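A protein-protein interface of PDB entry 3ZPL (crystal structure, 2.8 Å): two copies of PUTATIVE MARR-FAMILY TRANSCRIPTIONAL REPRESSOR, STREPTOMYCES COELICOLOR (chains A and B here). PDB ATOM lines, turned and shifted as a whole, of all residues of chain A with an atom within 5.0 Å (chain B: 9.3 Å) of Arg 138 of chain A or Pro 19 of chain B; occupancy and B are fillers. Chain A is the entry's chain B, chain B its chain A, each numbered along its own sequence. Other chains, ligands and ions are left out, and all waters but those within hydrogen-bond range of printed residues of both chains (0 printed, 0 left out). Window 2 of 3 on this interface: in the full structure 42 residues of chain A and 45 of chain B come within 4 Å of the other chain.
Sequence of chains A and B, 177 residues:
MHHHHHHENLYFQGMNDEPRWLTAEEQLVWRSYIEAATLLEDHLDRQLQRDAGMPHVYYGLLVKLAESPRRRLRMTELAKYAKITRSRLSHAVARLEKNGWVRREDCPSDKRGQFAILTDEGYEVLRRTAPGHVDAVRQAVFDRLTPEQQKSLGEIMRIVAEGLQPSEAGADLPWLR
The guanidinium group of Arg 20 of chain B is in salt-bridge range of the side-chain carboxylate of Asp 143 of chain A (3.8 Å).
NH2 of Arg 20 of chain B is in salt-bridge range of OE1 of Glu 26 of chain B.
O of Leu 22 of chain B sits at hydrogen-bond distance from NE2 of Gln 27 of chain B.
The side-chain carboxylate (OE1) of Glu 26 of chain B lies within hydrogen-bond range of the backbone NH (N) of Thr 23 of chain B, at 2.9 Å.
NH1 of Arg 138 of chain A lies within salt-bridge range of OD1 of Asp 135 of chain A, at 3.0 Å.
NH2 of Arg 138 of chain A is in salt-bridge range of OD2 of Asp 143 of chain A (2.7 Å).
Among the printed residues, merely in contact across the chains: Val 134 of chain A with Leu 22 of chain B (3.9 Å), Val 137 of chain A with Trp 30 of chain B (3.7 Å), Arg 138 of chain A with Pro 19 of chain B (3.8 Å), Arg 138 of chain A with Arg 20 of chain B (3.4 Å), Arg 138 of chain A with Leu 22 of chain B (3.3 Å), Phe 142 of chain A with Glu 26 of chain B (3.4 Å) and Phe 142 of chain A with Trp 30 of chain B (3.9 Å).
Of the printed residues of chain B, Val 134 of chain A touches Leu 22.
Asp 135 of chain A touches none of the printed residues of chain B.
Ala 136 of chain A touches none of the printed residues of chain B.
Val 137 of chain A touches just one residue of chain B: Trp 30.
Arg 138 of chain A touches just these residues of chain B: Pro 19, Arg 20 and Leu 22.
No residue of chain B comes within 4 Å of Ala 140 of chain A.
Of the printed residues of chain B, Phe 142 of chain A touches Glu 26 and Trp 30.
Of the printed residues of chain B, Asp 143 of chain A touches Arg 20.
Of the printed residues of chain A, Pro 19 of chain B touches Arg 138.
Of the printed residues of chain A, Arg 20 of chain B touches Arg 138 and Asp 143.
The nearest residue of chain B that does not touch Arg 138 of chain A is Trp 21 of chain B (5.0 Å).
The nearest residue of chain A that does not touch Pro 19 of chain B is Asp 135 of chain A (4.5 Å).
Hydrophobic or aromatic side chains of chain A within 4 Å of the printed part of chain B: Val 134, Val 137 and Phe 142.
Of the 9 printed residues of chain B, 5 touch a printed residue of chain A.
Hydrophobic or aromatic side chains of chain B within 4 Å of the printed part of chain A: Leu 22 and Trp 30.
Among the printed residues, 8 pairs touch across the chains.
No position is printed for both chains.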
ATOM      1  N   VAL A 134      19.812  24.130 -32.844  1.00  0.00           N
ATOM      2  CA  VAL A 134      19.347  23.362 -31.700  1.00  0.00           C
ATOM      3  C   VAL A 134      19.953  21.962 -31.711  1.00  0.00           C
ATOM      4  O   VAL A 134      20.492  21.528 -30.709  1.00  0.00           O
ATOM      5  CB  VAL A 134      17.802  23.345 -31.617  1.00  0.00           C
ATOM      6  CG1 VAL A 134      17.306  22.345 -30.578  1.00  0.00           C
ATOM      7  CG2 VAL A 134      17.305  24.734 -31.261  1.00  0.00           C
ATOM      8  N   ASP A 135      19.871  21.257 -32.837  1.00  0.00           N
ATOM      9  CA  ASP A 135      20.526  19.947 -32.988  1.00  0.00           C
ATOM     10  C   ASP A 135      21.961  20.008 -32.490  1.00  0.00           C
ATOM     11  O   ASP A 135      22.347  19.254 -31.599  1.00  0.00           O
ATOM     12  CB  ASP A 135      20.574  19.494 -34.466  1.00  0.00           C
ATOM     13  CG  ASP A 135      19.293  18.887 -34.947  1.00  0.00           C
ATOM     14  OD1 ASP A 135      18.301  18.965 -34.220  1.00  0.00           O
ATOM     15  OD2 ASP A 135      19.275  18.381 -36.091  1.00  0.00           O
ATOM     16  N   ALA A 136      22.743  20.897 -33.093  1.00  0.00           N
ATOM     17  CA  ALA A 136      24.170  21.025 -32.769  1.00  0.00           C
ATOM     18  C   ALA A 136      24.409  21.215 -31.267  1.00  0.00           C
ATOM     19  O   ALA A 136      25.334  20.643 -30.715  1.00  0.00           O
ATOM     20  CB  ALA A 136      24.795  22.168 -33.563  1.00  0.00           C
ATOM     21  N   VAL A 137      23.553  21.997 -30.621  1.00  0.00           N
ATOM     22  CA  VAL A 137      23.626  22.212 -29.184  1.00  0.00           C
ATOM     23  C   VAL A 137      23.142  20.992 -28.393  1.00  0.00           C
ATOM     24  O   VAL A 137      23.647  20.721 -27.313  1.00  0.00           O
ATOM     25  CB  VAL A 137      22.816  23.462 -28.774  1.00  0.00           C
ATOM     26  CG1 VAL A 137      22.699  23.572 -27.257  1.00  0.00           C
ATOM     27  CG2 VAL A 137      23.482  24.712 -29.336  1.00  0.00           C
ATOM     28  N   ARG A 138      22.154  20.269 -28.915  1.00  0.00           N
ATOM     29  CA  ARG A 138      21.767  19.007 -28.327  1.00  0.00           C
ATOM     30  C   ARG A 138      22.900  18.000 -28.369  1.00  0.00           C
ATOM     31  O   ARG A 138      23.307  17.471 -27.341  1.00  0.00           O
ATOM     32  CB  ARG A 138      20.599  18.395 -29.082  1.00  0.00           C
ATOM     33  CG  ARG A 138      19.242  18.869 -28.648  1.00  0.00           C
ATOM     34  CD  ARG A 138      18.212  17.903 -29.241  1.00  0.00           C
ATOM     35  NE  ARG A 138      18.781  16.604 -29.659  1.00  0.00           N
ATOM     36  CZ  ARG A 138      19.095  16.220 -30.912  1.00  0.00           C
ATOM     37  NH1 ARG A 138      18.882  16.997 -31.981  1.00  0.00           N
ATOM     38  NH2 ARG A 138      19.632  15.014 -31.107  1.00  0.00           N
ATOM     39  N   GLN A 139      23.397  17.744 -29.584  1.00  0.00           N
ATOM     40  CA  GLN A 139      24.333  16.652 -29.847  1.00  0.00           C
ATOM     41  C   GLN A 139      25.636  16.851 -29.100  1.00  0.00           C
ATOM     42  O   GLN A 139      26.181  15.901 -28.530  1.00  0.00           O
ATOM     43  CB  GLN A 139      24.519  16.481 -31.352  1.00  0.00           C
ATOM     44  CG  GLN A 139      23.301  15.800 -31.969  1.00  0.00           C
ATOM     45  CD  GLN A 139      23.335  15.712 -33.479  1.00  0.00           C
ATOM     46  OE1 GLN A 139      23.983  16.512 -34.154  1.00  0.00           O
ATOM     47  NE2 GLN A 139      22.584  14.760 -34.022  1.00  0.00           N
ATOM     48  N   ALA A 140      26.084  18.099 -29.014  1.00  0.00           N
ATOM     49  CA  ALA A 140      27.296  18.429 -28.282  1.00  0.00           C
ATOM     50  C   ALA A 140      27.124  18.344 -26.765  1.00  0.00           C
ATOM     51  O   ALA A 140      28.084  18.045 -26.057  1.00  0.00           O
ATOM     52  CB  ALA A 140      27.764  19.825 -28.668  1.00  0.00           C
ATOM     53  N   VAL A 141      25.927  18.632 -26.263  1.00  0.00           N
ATOM     54  CA  VAL A 141      25.729  18.800 -24.821  1.00  0.00           C
ATOM     55  C   VAL A 141      24.633  17.916 -24.243  1.00  0.00           C
ATOM     56  O   VAL A 141      24.923  16.914 -23.606  1.00  0.00           O
ATOM     57  CB  VAL A 141      25.434  20.276 -24.472  1.00  0.00           C
ATOM     58  CG1 VAL A 141      25.179  20.443 -22.981  1.00  0.00           C
ATOM     59  CG2 VAL A 141      26.587  21.155 -24.913  1.00  0.00           C
ATOM     60  N   PHE A 142      23.372  18.267 -24.480  1.00  0.00           N
ATOM     61  CA  PHE A 142      22.257  17.688 -23.701  1.00  0.00           C
ATOM     62  C   PHE A 142      22.025  16.197 -23.903  1.00  0.00           C
ATOM     63  O   PHE A 142      21.748  15.483 -22.946  1.00  0.00           O
ATOM     64  CB  PHE A 142      20.986  18.498 -23.920  1.00  0.00           C
ATOM     65  CG  PHE A 142      21.096  19.900 -23.387  1.00  0.00           C
ATOM     66  CD1 PHE A 142      20.946  20.151 -22.030  1.00  0.00           C
ATOM     67  CD2 PHE A 142      21.380  20.951 -24.227  1.00  0.00           C
ATOM     68  CE1 PHE A 142      21.046  21.427 -21.528  1.00  0.00           C
ATOM     69  CE2 PHE A 142      21.483  22.238 -23.731  1.00  0.00           C
ATOM     70  CZ  PHE A 142      21.321  22.475 -22.380  1.00  0.00           C
ATOM     71  N   ASP A 143      22.175  15.720 -25.132  1.00  0.00           N
ATOM     72  CA  ASP A 143      22.111  14.290 -25.398  1.00  0.00           C
ATOM     73  C   ASP A 143      23.175  13.477 -24.648  1.00  0.00           C
ATOM     74  O   ASP A 143      23.070  12.258 -24.582  1.00  0.00           O
ATOM     75  CB  ASP A 143      22.253  14.014 -26.896  1.00  0.00           C
ATOM     76  CG  ASP A 143      20.980  14.292 -27.670  1.00  0.00           C
ATOM     77  OD1 ASP A 143      19.891  14.438 -27.048  1.00  0.00           O
ATOM     78  OD2 ASP A 143      21.085  14.373 -28.924  1.00  0.00           O
ATOM     79  N   ARG A 144      24.186  14.137 -24.082  1.00  0.00           N
ATOM     80  CA  ARG A 144      25.314  13.450 -23.422  1.00  0.00           C
ATOM     81  C   ARG A 144      25.293  13.499 -21.891  1.00  0.00           C
ATOM     82  O   ARG A 144      26.154  12.892 -21.245  1.00  0.00           O
ATOM     83  CB  ARG A 144      26.639  14.048 -23.905  1.00  0.00           C
ATOM     84  CG  ARG A 144      26.748  14.119 -25.420  1.00  0.00           C
ATOM     85  CD  ARG A 144      28.174  14.399 -25.878  1.00  0.00           C
ATOM     86  NE  ARG A 144      28.646  13.393 -26.827  1.00  0.00           N
ATOM     87  CZ  ARG A 144      29.066  13.626 -28.070  1.00  0.00           C
ATOM     88  NH1 ARG A 144      29.103  14.863 -28.584  1.00  0.00           N
ATOM     89  NH2 ARG A 144      29.476  12.598 -28.812  1.00  0.00           N
ATOM     90  N   PRO B  19      16.052  13.923 -33.230  1.00  0.00           N
ATOM     91  CA  PRO B  19      15.793  15.342 -33.527  1.00  0.00           C
ATOM     92  C   PRO B  19      14.575  15.917 -32.743  1.00  0.00           C
ATOM     93  O   PRO B  19      13.549  16.363 -33.290  1.00  0.00           O
ATOM     94  CB  PRO B  19      15.656  15.362 -35.068  1.00  0.00           C
ATOM     95  CG  PRO B  19      15.369  13.953 -35.450  1.00  0.00           C
ATOM     96  CD  PRO B  19      16.118  13.109 -34.454  1.00  0.00           C
ATOM     97  N   ARG B  20      14.745  15.916 -31.430  1.00  0.00           N
ATOM     98  CA  ARG B  20      13.743  16.369 -30.462  1.00  0.00           C
ATOM     99  C   ARG B  20      13.815  17.883 -30.194  1.00  0.00           C
ATOM    100  O   ARG B  20      14.598  18.571 -30.832  1.00  0.00           O
ATOM    101  CB  ARG B  20      13.958  15.611 -29.150  1.00  0.00           C
ATOM    102  CG  ARG B  20      15.375  15.712 -28.612  1.00  0.00           C
ATOM    103  CD  ARG B  20      15.564  15.000 -27.303  1.00  0.00           C
ATOM    104  NE  ARG B  20      15.195  15.836 -26.156  1.00  0.00           N
ATOM    105  CZ  ARG B  20      15.983  16.772 -25.616  1.00  0.00           C
ATOM    106  NH1 ARG B  20      17.198  17.006 -26.101  1.00  0.00           N
ATOM    107  NH2 ARG B  20      15.556  17.485 -24.581  1.00  0.00           N
ATOM    108  N   TRP B  21      13.009  18.378 -29.247  1.00  0.00           N
ATOM    109  CA  TRP B  21      12.962  19.799 -28.850  1.00  0.00           C
ATOM    110  C   TRP B  21      13.699  19.936 -27.541  1.00  0.00           C
ATOM    111  O   TRP B  21      13.958  18.937 -26.887  1.00  0.00           O
ATOM    112  CB  TRP B  21      11.521  20.259 -28.561  1.00  0.00           C
ATOM    113  CG  TRP B  21      10.683  20.694 -29.716  1.00  0.00           C
ATOM    114  CD1 TRP B  21      10.951  20.510 -31.037  1.00  0.00           C
ATOM    115  CD2 TRP B  21       9.385  21.316 -29.655  1.00  0.00           C
ATOM    116  NE1 TRP B  21       9.925  20.999 -31.808  1.00  0.00           N
ATOM    117  CE2 TRP B  21       8.950  21.502 -30.986  1.00  0.00           C
ATOM    118  CE3 TRP B  21       8.556  21.754 -28.607  1.00  0.00           C
ATOM    119  CZ2 TRP B  21       7.716  22.094 -31.301  1.00  0.00           C
ATOM    120  CZ3 TRP B  21       7.340  22.349 -28.920  1.00  0.00           C
ATOM    121  CH2 TRP B  21       6.931  22.507 -30.259  1.00  0.00           C
ATOM    122  N   LEU B  22      14.001  21.173 -27.140  1.00  0.00           N
ATOM    123  CA  LEU B  22      14.613  21.421 -25.835  1.00  0.00           C
ATOM    124  C   LEU B  22      13.582  21.826 -24.825  1.00  0.00           C
ATOM    125  O   LEU B  22      12.816  22.748 -25.067  1.00  0.00           O
ATOM    126  CB  LEU B  22      15.667  22.530 -25.915  1.00  0.00           C
ATOM    127  CG  LEU B  22      17.118  22.097 -25.876  1.00  0.00           C
ATOM    128  CD1 LEU B  22      17.407  21.057 -26.950  1.00  0.00           C
ATOM    129  CD2 LEU B  22      17.996  23.331 -26.029  1.00  0.00           C
ATOM    130  N   THR B  23      13.584  21.177 -23.665  1.00  0.00           N
ATOM    131  CA  THR B  23      12.645  21.575 -22.611  1.00  0.00           C
ATOM    132  C   THR B  23      12.982  22.994 -22.210  1.00  0.00           C
ATOM    133  O   THR B  23      14.067  23.471 -22.472  1.00  0.00           O
ATOM    134  CB  THR B  23      12.689  20.666 -21.360  1.00  0.00           C
ATOM    135  OG1 THR B  23      13.895  20.903 -20.617  1.00  0.00           O
ATOM    136  CG2 THR B  23      12.584  19.188 -21.744  1.00  0.00           C
ATOM    137  N   GLU B  26      16.051  22.917 -19.944  1.00  0.00           N
ATOM    138  CA  GLU B  26      17.288  22.805 -20.733  1.00  0.00           C
ATOM    139  C   GLU B  26      17.668  24.116 -21.386  1.00  0.00           C
ATOM    140  O   GLU B  26      18.821  24.538 -21.332  1.00  0.00           O
ATOM    141  CB  GLU B  26      17.151  21.713 -21.789  1.00  0.00           C
ATOM    142  CG  GLU B  26      17.141  20.287 -21.231  1.00  0.00           C
ATOM    143  CD  GLU B  26      16.781  19.261 -22.292  1.00  0.00           C
ATOM    144  OE1 GLU B  26      15.834  19.521 -23.071  1.00  0.00           O
ATOM    145  OE2 GLU B  26      17.441  18.201 -22.378  1.00  0.00           O
ATOM    146  N   GLN B  27      16.684  24.775 -21.974  1.00  0.00           N
ATOM    147  CA  GLN B  27      16.905  26.088 -22.542  1.00  0.00           C
ATOM    148  C   GLN B  27      17.559  27.039 -21.524  1.00  0.00           C
ATOM    149  O   GLN B  27      18.477  27.774 -21.874  1.00  0.00           O
ATOM    150  CB  GLN B  27      15.580  26.680 -23.033  1.00  0.00           C
ATOM    151  CG  GLN B  27      15.172  26.206 -24.416  1.00  0.00           C
ATOM    152  CD  GLN B  27      13.799  26.712 -24.813  1.00  0.00           C
ATOM    153  OE1 GLN B  27      13.617  27.917 -25.043  1.00  0.00           O
ATOM    154  NE2 GLN B  27      12.825  25.809 -24.901  1.00  0.00           N
ATOM    155  N   TRP B  30      21.230  26.139 -20.768  1.00  0.00           N
ATOM    156  CA  TRP B  30      22.032  26.617 -21.887  1.00  0.00           C
ATOM    157  C   TRP B  30      22.285  28.118 -21.814  1.00  0.00           C
ATOM    158  O   TRP B  30      23.411  28.570 -21.956  1.00  0.00           O
ATOM    159  CB  TRP B  30      21.347  26.252 -23.203  1.00  0.00           C
ATOM    160  CG  TRP B  30      22.110  26.665 -24.411  1.00  0.00           C
ATOM    161  CD1 TRP B  30      21.701  27.517 -25.387  1.00  0.00           C
ATOM    162  CD2 TRP B  30      23.432  26.254 -24.766  1.00  0.00           C
ATOM    163  NE1 TRP B  30      22.686  27.666 -26.332  1.00  0.00           N
ATOM    164  CE2 TRP B  30      23.756  26.888 -25.978  1.00  0.00           C
ATOM    165  CE3 TRP B  30      24.375  25.405 -24.175  1.00  0.00           C
ATOM    166  CZ2 TRP B  30      24.971  26.700 -26.614  1.00  0.00           C
ATOM    167  CZ3 TRP B  30      25.592  25.215 -24.817  1.00  0.00           C
ATOM    168  CH2 TRP B  30      25.878  25.866 -26.021  1.00  0.00           C
ATOM    169  N   VAL B 160      31.806  16.797 -22.593  1.00  0.00           N
ATOM    170  CA  VAL B 160      31.570  17.760 -23.667  1.00  0.00           C
ATOM    171  C   VAL B 160      32.809  17.871 -24.555  1.00  0.00           C
ATOM    172  O   VAL B 160      32.701  17.852 -25.778  1.00  0.00           O
ATOM    173  CB  VAL B 160      31.187  19.150 -23.103  1.00  0.00           C
ATOM    174  CG1 VAL B 160      31.226  20.218 -24.183  1.00  0.00           C
ATOM    175  CG2 VAL B 160      29.808  19.096 -22.463  1.00  0.00           C
